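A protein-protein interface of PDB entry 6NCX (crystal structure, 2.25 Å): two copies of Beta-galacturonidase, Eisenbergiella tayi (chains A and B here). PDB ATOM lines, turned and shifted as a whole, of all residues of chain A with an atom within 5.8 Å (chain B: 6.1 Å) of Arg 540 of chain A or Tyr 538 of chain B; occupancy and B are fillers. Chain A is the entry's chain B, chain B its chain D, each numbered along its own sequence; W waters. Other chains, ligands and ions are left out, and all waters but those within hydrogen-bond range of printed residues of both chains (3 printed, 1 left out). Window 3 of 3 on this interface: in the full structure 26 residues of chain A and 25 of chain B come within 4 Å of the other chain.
The side-chain amide oxygen (OE1) of Gln 283 of chain A sits at hydrogen-bond distance from a ring nitrogen (NE2) of His 281 of chain B. The side-chain amide nitrogen (NE2) of Gln 283 of chain A is in hydrogen-bond range of a ring nitrogen (ND1) of His 295 of chain B.
N of Gln 283 of chain B is in hydrogen-bond range of ND1 of His 281 of chain B. N of Tyr 538 of chain B lies close to OD1 of Asp 536 of chain B (3.1 Å). OD2 of Asp 536 of chain B lies within salt-bridge range of NH2 of Arg 540 of chain B (3.0 Å). The backbone NH (N) of Tyr 538 of chain A sits at hydrogen-bond distance from the side-chain carboxylate (OD1) of Asp 536 of chain A (3.1 Å). N of Arg 539 of chain A is in hydrogen-bond range of OD1 of Asp 536 of chain A, at 3.1 Å. The side-chain carboxylate (OD2) of Asp 536 of chain A is in salt-bridge range of the guanidinium group (NH2) of Arg 540 of chain A, 2.9 Å away.
Among the printed residues, merely in contact across the chains: Tyr 538 of chain A with Arg 540 of chain B (3.3 Å), Tyr 538 of chain A with Tyr 538 of chain B (3.3 Å), Arg 540 of chain A with Tyr 538 of chain B (3.6 Å), Arg 539 of chain A with Gln 283 of chain B (3.9 Å) and Arg 540 of chain A with Arg 540 of chain B (3.9 Å).
Printed residues of chain B within 4 Å of Arg 540 of chain A: Tyr 538 (3.6 Å) and Arg 540 (3.9 Å). Tyr 538 of chain B touches just these residues of chain A: Tyr 538 (3.3 Å) and Arg 540 (3.6 Å). Printed residues of chain A within 4 Å of His 281 of chain B: Gln 283. Of the printed residues of chain A, Arg 540 of chain B touches Tyr 538 and Arg 540. Of the printed residues of chain B, Tyr 538 of chain A touches Tyr 538 (3.3 Å) and Arg 540 (3.3 Å). Arg 539 of chain B touches none of the printed residues of chain A.
Printed residues of chain A that touch a printed residue of chain B: Gln 283, Tyr 538, Arg 539 and Arg 540. Printed residues of chain B that touch a printed residue of chain A: His 281, Gln 283, His 295, Tyr 538 and Arg 540. Among the printed residues, no Asp or Glu carboxylate lies within 4 Å of a Lys or Arg side-chain nitrogen of the other chain.
Tyr 538 of chain A touches its own counterpart, Tyr 538 of chain B. Tyr 538 of chain A touches Arg 540 of chain B, and with the chains exchanged Arg 540 of chain A touches Tyr 538 of chain B. Arg 539 of chain A touches Gln 283 of chain B, but with the chains exchanged Gln 283 of chain A does not touch Arg 539 of chain B (4.05 Å). Arg 540 of chain B touches its own counterpart, Arg 540 of chain A. 7 positions are printed for both chains. Of the 7 pairs that touch across the chains among the printed residues, 4 have their exchanged pair printed and touching as well.
Water W2 bridges OH of Tyr 538 of chain B (2.8 Å) and O of Tyr 538 of chain A (2.8 Å). Water W1 bridges NE2 of Gln 283 of chain A and NE of Arg 539 of chain B. Water W3 lies within hydrogen-bond range of the side-chain amide nitrogen (NE2) of Gln 283 of chain B (3.2 Å) and the guanidinium group (NE) of Arg 539 of chain A (3.3 Å).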
ATOM      1  N   GLN A 283     -23.092 -19.258 -20.755  1.00  0.00           N
ATOM      2  CA  GLN A 283     -23.011 -18.197 -21.747  1.00  0.00           C
ATOM      3  C   GLN A 283     -21.838 -18.370 -22.695  1.00  0.00           C
ATOM      4  O   GLN A 283     -21.877 -17.866 -23.822  1.00  0.00           O
ATOM      5  CB  GLN A 283     -22.881 -16.818 -21.086  1.00  0.00           C
ATOM      6  CG  GLN A 283     -24.091 -16.293 -20.340  1.00  0.00           C
ATOM      7  CD  GLN A 283     -23.873 -14.844 -19.882  1.00  0.00           C
ATOM      8  OE1 GLN A 283     -23.471 -14.577 -18.725  1.00  0.00           O
ATOM      9  NE2 GLN A 283     -24.108 -13.902 -20.799  1.00  0.00           N
ATOM     10  N   TYR A 472     -30.521 -27.717  -8.520  1.00  0.00           N
ATOM     11  CA  TYR A 472     -30.684 -26.466  -7.800  1.00  0.00           C
ATOM     12  C   TYR A 472     -32.141 -26.062  -7.853  1.00  0.00           C
ATOM     13  O   TYR A 472     -32.781 -26.137  -8.905  1.00  0.00           O
ATOM     14  CB  TYR A 472     -29.802 -25.361  -8.398  1.00  0.00           C
ATOM     15  CG  TYR A 472     -29.919 -24.020  -7.689  1.00  0.00           C
ATOM     16  CD1 TYR A 472     -30.635 -22.971  -8.253  1.00  0.00           C
ATOM     17  CD2 TYR A 472     -29.315 -23.810  -6.449  1.00  0.00           C
ATOM     18  CE1 TYR A 472     -30.745 -21.745  -7.614  1.00  0.00           C
ATOM     19  CE2 TYR A 472     -29.425 -22.587  -5.787  1.00  0.00           C
ATOM     20  CZ  TYR A 472     -30.136 -21.558  -6.379  1.00  0.00           C
ATOM     21  OH  TYR A 472     -30.243 -20.341  -5.729  1.00  0.00           O
ATOM     22  N   ILE A 534     -21.200 -28.443  -7.056  1.00  0.00           N
ATOM     23  CA  ILE A 534     -21.456 -27.850  -5.745  1.00  0.00           C
ATOM     24  C   ILE A 534     -22.094 -26.482  -5.933  1.00  0.00           C
ATOM     25  O   ILE A 534     -22.869 -26.007  -5.095  1.00  0.00           O
ATOM     26  CB  ILE A 534     -20.144 -27.778  -4.938  1.00  0.00           C
ATOM     27  CG1 ILE A 534     -19.550 -29.177  -4.779  1.00  0.00           C
ATOM     28  CG2 ILE A 534     -20.384 -27.123  -3.569  1.00  0.00           C
ATOM     29  CD1 ILE A 534     -20.499 -30.165  -4.050  1.00  0.00           C
ATOM     30  N   VAL A 535     -21.781 -25.849  -7.045  1.00  0.00           N
ATOM     31  CA  VAL A 535     -22.427 -24.648  -7.541  1.00  0.00           C
ATOM     32  C   VAL A 535     -23.165 -25.043  -8.823  1.00  0.00           C
ATOM     33  O   VAL A 535     -22.801 -26.026  -9.472  1.00  0.00           O
ATOM     34  CB  VAL A 535     -21.305 -23.599  -7.726  1.00  0.00           C
ATOM     35  CG1 VAL A 535     -20.921 -23.374  -9.204  1.00  0.00           C
ATOM     36  CG2 VAL A 535     -21.583 -22.338  -6.947  1.00  0.00           C
ATOM     37  N   ASP A 536     -24.256 -24.351  -9.154  1.00  0.00           N
ATOM     38  CA  ASP A 536     -24.958 -24.751 -10.375  1.00  0.00           C
ATOM     39  C   ASP A 536     -24.306 -24.070 -11.587  1.00  0.00           C
ATOM     40  O   ASP A 536     -23.287 -23.389 -11.462  1.00  0.00           O
ATOM     41  CB  ASP A 536     -26.463 -24.481 -10.252  1.00  0.00           C
ATOM     42  CG  ASP A 536     -26.854 -23.046 -10.562  1.00  0.00           C
ATOM     43  OD1 ASP A 536     -26.010 -22.122 -10.465  1.00  0.00           O
ATOM     44  OD2 ASP A 536     -28.041 -22.847 -10.885  1.00  0.00           O
ATOM     45  N   GLU A 537     -24.877 -24.266 -12.784  1.00  0.00           N
ATOM     46  CA  GLU A 537     -24.224 -23.783 -14.000  1.00  0.00           C
ATOM     47  C   GLU A 537     -24.111 -22.264 -14.029  1.00  0.00           C
ATOM     48  O   GLU A 537     -23.217 -21.729 -14.696  1.00  0.00           O
ATOM     49  CB  GLU A 537     -24.961 -24.267 -15.250  1.00  0.00           C
ATOM     50  CG  GLU A 537     -26.377 -23.694 -15.432  1.00  0.00           C
ATOM     51  CD  GLU A 537     -27.468 -24.652 -14.956  1.00  0.00           C
ATOM     52  OE1 GLU A 537     -27.258 -25.387 -13.943  1.00  0.00           O
ATOM     53  OE2 GLU A 537     -28.539 -24.681 -15.610  1.00  0.00           O
ATOM     54  N   TYR A 538     -24.975 -21.560 -13.305  1.00  0.00           N
ATOM     55  CA  TYR A 538     -24.879 -20.120 -13.162  1.00  0.00           C
ATOM     56  C   TYR A 538     -24.037 -19.716 -11.968  1.00  0.00           C
ATOM     57  O   TYR A 538     -23.985 -18.533 -11.645  1.00  0.00           O
ATOM     58  CB  TYR A 538     -26.282 -19.511 -13.065  1.00  0.00           C
ATOM     59  CG  TYR A 538     -27.042 -19.675 -14.363  1.00  0.00           C
ATOM     60  CD1 TYR A 538     -26.754 -18.850 -15.451  1.00  0.00           C
ATOM     61  CD2 TYR A 538     -28.024 -20.669 -14.523  1.00  0.00           C
ATOM     62  CE1 TYR A 538     -27.428 -18.979 -16.664  1.00  0.00           C
ATOM     63  CE2 TYR A 538     -28.690 -20.803 -15.732  1.00  0.00           C
ATOM     64  CZ  TYR A 538     -28.378 -19.945 -16.797  1.00  0.00           C
ATOM     65  OH  TYR A 538     -29.009 -20.038 -18.004  1.00  0.00           O
ATOM     66  N   ARG A 539     -23.374 -20.675 -11.315  1.00  0.00           N
ATOM     67  CA  ARG A 539     -22.492 -20.448 -10.174  1.00  0.00           C
ATOM     68  C   ARG A 539     -23.253 -20.070  -8.902  1.00  0.00           C
ATOM     69  O   ARG A 539     -22.688 -19.448  -7.992  1.00  0.00           O
ATOM     70  CB  ARG A 539     -21.413 -19.397 -10.496  1.00  0.00           C
ATOM     71  CG  ARG A 539     -20.206 -19.962 -11.203  1.00  0.00           C
ATOM     72  CD  ARG A 539     -20.497 -20.528 -12.604  1.00  0.00           C
ATOM     73  NE  ARG A 539     -19.260 -21.028 -13.190  1.00  0.00           N
ATOM     74  CZ  ARG A 539     -19.183 -21.845 -14.237  1.00  0.00           C
ATOM     75  NH1 ARG A 539     -20.279 -22.275 -14.845  1.00  0.00           N
ATOM     76  NH2 ARG A 539     -17.997 -22.241 -14.669  1.00  0.00           N
ATOM     77  N   ARG A 540     -24.512 -20.452  -8.809  1.00  0.00           N
ATOM     78  CA  ARG A 540     -25.259 -20.264  -7.573  1.00  0.00           C
ATOM     79  C   ARG A 540     -24.939 -21.395  -6.600  1.00  0.00           C
ATOM     80  O   ARG A 540     -25.042 -22.569  -6.970  1.00  0.00           O
ATOM     81  CB  ARG A 540     -26.762 -20.202  -7.867  1.00  0.00           C
ATOM     82  CG  ARG A 540     -27.143 -18.945  -8.671  1.00  0.00           C
ATOM     83  CD  ARG A 540     -28.598 -18.911  -9.081  1.00  0.00           C
ATOM     84  NE  ARG A 540     -28.919 -19.944 -10.050  1.00  0.00           N
ATOM     85  CZ  ARG A 540     -30.105 -20.080 -10.634  1.00  0.00           C
ATOM     86  NH1 ARG A 540     -31.084 -19.219 -10.362  1.00  0.00           N
ATOM     87  NH2 ARG A 540     -30.303 -21.060 -11.501  1.00  0.00           N
ATOM     88  N   PRO A 541     -24.526 -21.086  -5.369  1.00  0.00           N
ATOM     89  CA  PRO A 541     -24.191 -22.150  -4.402  1.00  0.00           C
ATOM     90  C   PRO A 541     -25.401 -22.995  -4.010  1.00  0.00           C
ATOM     91  O   PRO A 541     -26.428 -22.481  -3.562  1.00  0.00           O
ATOM     92  CB  PRO A 541     -23.636 -21.374  -3.199  1.00  0.00           C
ATOM     93  CG  PRO A 541     -24.187 -19.974  -3.362  1.00  0.00           C
ATOM     94  CD  PRO A 541     -24.222 -19.746  -4.843  1.00  0.00           C
ATOM     95  N   LYS A 542     -25.263 -24.306  -4.167  1.00  0.00           N
ATOM     96  CA  LYS A 542     -26.256 -25.218  -3.642  1.00  0.00           C
ATOM     97  C   LYS A 542     -26.090 -25.337  -2.127  1.00  0.00           C
ATOM     98  O   LYS A 542     -25.124 -24.826  -1.544  1.00  0.00           O
ATOM     99  CB  LYS A 542     -26.131 -26.583  -4.324  1.00  0.00           C
ATOM    100  CG  LYS A 542     -26.512 -26.571  -5.798  1.00  0.00           C
ATOM    101  CD  LYS A 542     -26.182 -27.906  -6.487  1.00  0.00           C
ATOM    102  CE  LYS A 542     -26.418 -27.801  -7.994  1.00  0.00           C
ATOM    103  NZ  LYS A 542     -25.744 -28.895  -8.721  1.00  0.00           N
ATOM    104  N   HIS B 281     -24.457  -7.438 -14.441  1.00  0.00           N
ATOM    105  CA  HIS B 281     -24.387  -8.872 -14.681  1.00  0.00           C
ATOM    106  C   HIS B 281     -24.190  -9.596 -13.350  1.00  0.00           C
ATOM    107  O   HIS B 281     -23.402  -9.135 -12.510  1.00  0.00           O
ATOM    108  CB  HIS B 281     -23.254  -9.225 -15.666  1.00  0.00           C
ATOM    109  CG  HIS B 281     -23.215 -10.671 -16.046  1.00  0.00           C
ATOM    110  ND1 HIS B 281     -22.720 -11.645 -15.210  1.00  0.00           N
ATOM    111  CD2 HIS B 281     -23.648 -11.315 -17.156  1.00  0.00           C
ATOM    112  CE1 HIS B 281     -22.822 -12.824 -15.795  1.00  0.00           C
ATOM    113  NE2 HIS B 281     -23.383 -12.653 -16.977  1.00  0.00           N
ATOM    114  N   PRO B 282     -24.875 -10.724 -13.137  1.00  0.00           N
ATOM    115  CA  PRO B 282     -24.799 -11.402 -11.830  1.00  0.00           C
ATOM    116  C   PRO B 282     -23.410 -11.900 -11.442  1.00  0.00           C
ATOM    117  O   PRO B 282     -23.169 -12.131 -10.253  1.00  0.00           O
ATOM    118  CB  PRO B 282     -25.787 -12.567 -11.992  1.00  0.00           C
ATOM    119  CG  PRO B 282     -25.951 -12.727 -13.461  1.00  0.00           C
ATOM    120  CD  PRO B 282     -25.828 -11.371 -14.041  1.00  0.00           C
ATOM    121  N   GLN B 283     -22.485 -12.072 -12.385  1.00  0.00           N
ATOM    122  CA  GLN B 283     -21.115 -12.431 -12.018  1.00  0.00           C
ATOM    123  C   GLN B 283     -20.135 -11.269 -12.108  1.00  0.00           C
ATOM    124  O   GLN B 283     -19.103 -11.279 -11.418  1.00  0.00           O
ATOM    125  CB  GLN B 283     -20.592 -13.566 -12.902  1.00  0.00           C
ATOM    126  CG  GLN B 283     -21.293 -14.892 -12.736  1.00  0.00           C
ATOM    127  CD  GLN B 283     -20.641 -15.959 -13.594  1.00  0.00           C
ATOM    128  OE1 GLN B 283     -21.063 -16.203 -14.731  1.00  0.00           O
ATOM    129  NE2 GLN B 283     -19.584 -16.586 -13.070  1.00  0.00           N
ATOM    130  N   HIS B 295     -22.269 -11.184 -25.988  1.00  0.00           N
ATOM    131  CA  HIS B 295     -23.392 -12.083 -25.784  1.00  0.00           C
ATOM    132  C   HIS B 295     -24.690 -11.285 -25.665  1.00  0.00           C
ATOM    133  O   HIS B 295     -25.690 -11.605 -26.318  1.00  0.00           O
ATOM    134  CB  HIS B 295     -23.142 -12.970 -24.559  1.00  0.00           C
ATOM    135  CG  HIS B 295     -24.154 -14.061 -24.399  1.00  0.00           C
ATOM    136  ND1 HIS B 295     -25.238 -13.956 -23.556  1.00  0.00           N
ATOM    137  CD2 HIS B 295     -24.274 -15.260 -25.017  1.00  0.00           C
ATOM    138  CE1 HIS B 295     -25.969 -15.046 -23.645  1.00  0.00           C
ATOM    139  NE2 HIS B 295     -25.415 -15.846 -24.536  1.00  0.00           N
ATOM    140  N   ARG B 527     -36.946  -9.308  -5.207  1.00  0.00           N
ATOM    141  CA  ARG B 527     -35.607  -9.889  -5.198  1.00  0.00           C
ATOM    142  C   ARG B 527     -34.504  -8.836  -5.113  1.00  0.00           C
ATOM    143  O   ARG B 527     -33.330  -9.161  -5.342  1.00  0.00           O
ATOM    144  CB  ARG B 527     -35.369 -10.778  -6.435  1.00  0.00           C
ATOM    145  CG  ARG B 527     -36.537 -11.679  -6.834  1.00  0.00           C
ATOM    146  CD  ARG B 527     -36.184 -12.483  -8.076  1.00  0.00           C
ATOM    147  NE  ARG B 527     -35.852 -11.628  -9.215  1.00  0.00           N
ATOM    148  CZ  ARG B 527     -34.937 -11.935 -10.145  1.00  0.00           C
ATOM    149  NH1 ARG B 527     -34.238 -13.073 -10.054  1.00  0.00           N
ATOM    150  NH2 ARG B 527     -34.691 -11.094 -11.160  1.00  0.00           N
ATOM    151  N   VAL B 535     -34.886 -10.516 -20.892  1.00  0.00           N
ATOM    152  CA  VAL B 535     -34.138 -11.657 -20.382  1.00  0.00           C
ATOM    153  C   VAL B 535     -33.909 -11.389 -18.905  1.00  0.00           C
ATOM    154  O   VAL B 535     -33.915 -10.233 -18.473  1.00  0.00           O
ATOM    155  CB  VAL B 535     -32.795 -11.902 -21.124  1.00  0.00           C
ATOM    156  CG1 VAL B 535     -33.016 -12.036 -22.613  1.00  0.00           C
ATOM    157  CG2 VAL B 535     -31.796 -10.794 -20.851  1.00  0.00           C
ATOM    158  N   ASP B 536     -33.757 -12.455 -18.116  1.00  0.00           N
ATOM    159  CA  ASP B 536     -33.490 -12.241 -16.702  1.00  0.00           C
ATOM    160  C   ASP B 536     -31.995 -11.970 -16.536  1.00  0.00           C
ATOM    161  O   ASP B 536     -31.259 -11.890 -17.517  1.00  0.00           O
ATOM    162  CB  ASP B 536     -34.010 -13.417 -15.865  1.00  0.00           C
ATOM    163  CG  ASP B 536     -33.072 -14.629 -15.864  1.00  0.00           C
ATOM    164  OD1 ASP B 536     -32.280 -14.829 -16.830  1.00  0.00           O
ATOM    165  OD2 ASP B 536     -33.140 -15.396 -14.873  1.00  0.00           O
ATOM    166  N   GLU B 537     -31.531 -11.812 -15.288  1.00  0.00           N
ATOM    167  CA  GLU B 537     -30.142 -11.407 -15.073  1.00  0.00           C
ATOM    168  C   GLU B 537     -29.161 -12.442 -15.619  1.00  0.00           C
ATOM    169  O   GLU B 537     -28.034 -12.101 -16.003  1.00  0.00           O
ATOM    170  CB  GLU B 537     -29.898 -11.138 -13.585  1.00  0.00           C
ATOM    171  CG  GLU B 537     -29.939 -12.363 -12.679  1.00  0.00           C
ATOM    172  CD  GLU B 537     -31.328 -12.719 -12.149  1.00  0.00           C
ATOM    173  OE1 GLU B 537     -32.350 -12.360 -12.778  1.00  0.00           O
ATOM    174  OE2 GLU B 537     -31.403 -13.379 -11.089  1.00  0.00           O
ATOM    175  N   TYR B 538     -29.575 -13.697 -15.710  1.00  0.00           N
ATOM    176  CA  TYR B 538     -28.714 -14.729 -16.264  1.00  0.00           C
ATOM    177  C   TYR B 538     -28.857 -14.841 -17.776  1.00  0.00           C
ATOM    178  O   TYR B 538     -28.338 -15.788 -18.369  1.00  0.00           O
ATOM    179  CB  TYR B 538     -28.993 -16.062 -15.549  1.00  0.00           C
ATOM    180  CG  TYR B 538     -28.561 -15.975 -14.101  1.00  0.00           C
ATOM    181  CD1 TYR B 538     -27.222 -16.007 -13.762  1.00  0.00           C
ATOM    182  CD2 TYR B 538     -29.486 -15.811 -13.078  1.00  0.00           C
ATOM    183  CE1 TYR B 538     -26.793 -15.906 -12.436  1.00  0.00           C
ATOM    184  CE2 TYR B 538     -29.074 -15.708 -11.731  1.00  0.00           C
ATOM    185  CZ  TYR B 538     -27.721 -15.751 -11.426  1.00  0.00           C
ATOM    186  OH  TYR B 538     -27.281 -15.648 -10.120  1.00  0.00           O
ATOM    187  N   ARG B 539     -29.524 -13.866 -18.403  1.00  0.00           N
ATOM    188  CA  ARG B 539     -29.713 -13.778 -19.851  1.00  0.00           C
ATOM    189  C   ARG B 539     -30.583 -14.911 -20.391  1.00  0.00           C
ATOM    190  O   ARG B 539     -30.455 -15.306 -21.559  1.00  0.00           O
ATOM    191  CB  ARG B 539     -28.371 -13.719 -20.595  1.00  0.00           C
ATOM    192  CG  ARG B 539     -27.829 -12.304 -20.803  1.00  0.00           C
ATOM    193  CD  ARG B 539     -27.753 -11.507 -19.514  1.00  0.00           C
ATOM    194  NE  ARG B 539     -26.927 -10.322 -19.673  1.00  0.00           N
ATOM    195  CZ  ARG B 539     -26.547  -9.515 -18.683  1.00  0.00           C
ATOM    196  NH1 ARG B 539     -26.921  -9.750 -17.430  1.00  0.00           N
ATOM    197  NH2 ARG B 539     -25.790  -8.457 -18.957  1.00  0.00           N
ATOM    198  N   ARG B 540     -31.467 -15.448 -19.542  1.00  0.00           N
ATOM    199  CA  ARG B 540     -32.472 -16.410 -20.007  1.00  0.00           C
ATOM    200  C   ARG B 540     -33.693 -15.649 -20.522  1.00  0.00           C
ATOM    201  O   ARG B 540     -34.168 -14.727 -19.846  1.00  0.00           O
ATOM    202  CB  ARG B 540     -32.871 -17.385 -18.882  1.00  0.00           C
ATOM    203  CG  ARG B 540     -31.693 -18.189 -18.334  1.00  0.00           C
ATOM    204  CD  ARG B 540     -32.083 -19.092 -17.175  1.00  0.00           C
ATOM    205  NE  ARG B 540     -32.454 -18.339 -15.973  1.00  0.00           N
ATOM    206  CZ  ARG B 540     -32.649 -18.893 -14.776  1.00  0.00           C
ATOM    207  NH1 ARG B 540     -32.504 -20.205 -14.622  1.00  0.00           N
ATOM    208  NH2 ARG B 540     -32.983 -18.143 -13.735  1.00  0.00           N
HETATM  209  O   HOH W   1     -23.852 -10.961 -20.771  1.00  0.00           O
HETATM  210  O   HOH W   2     -24.608 -16.385  -9.967  1.00  0.00           O
HETATM  211  O   HOH W   3     -17.315 -18.493 -14.187  1.00  0.00           O
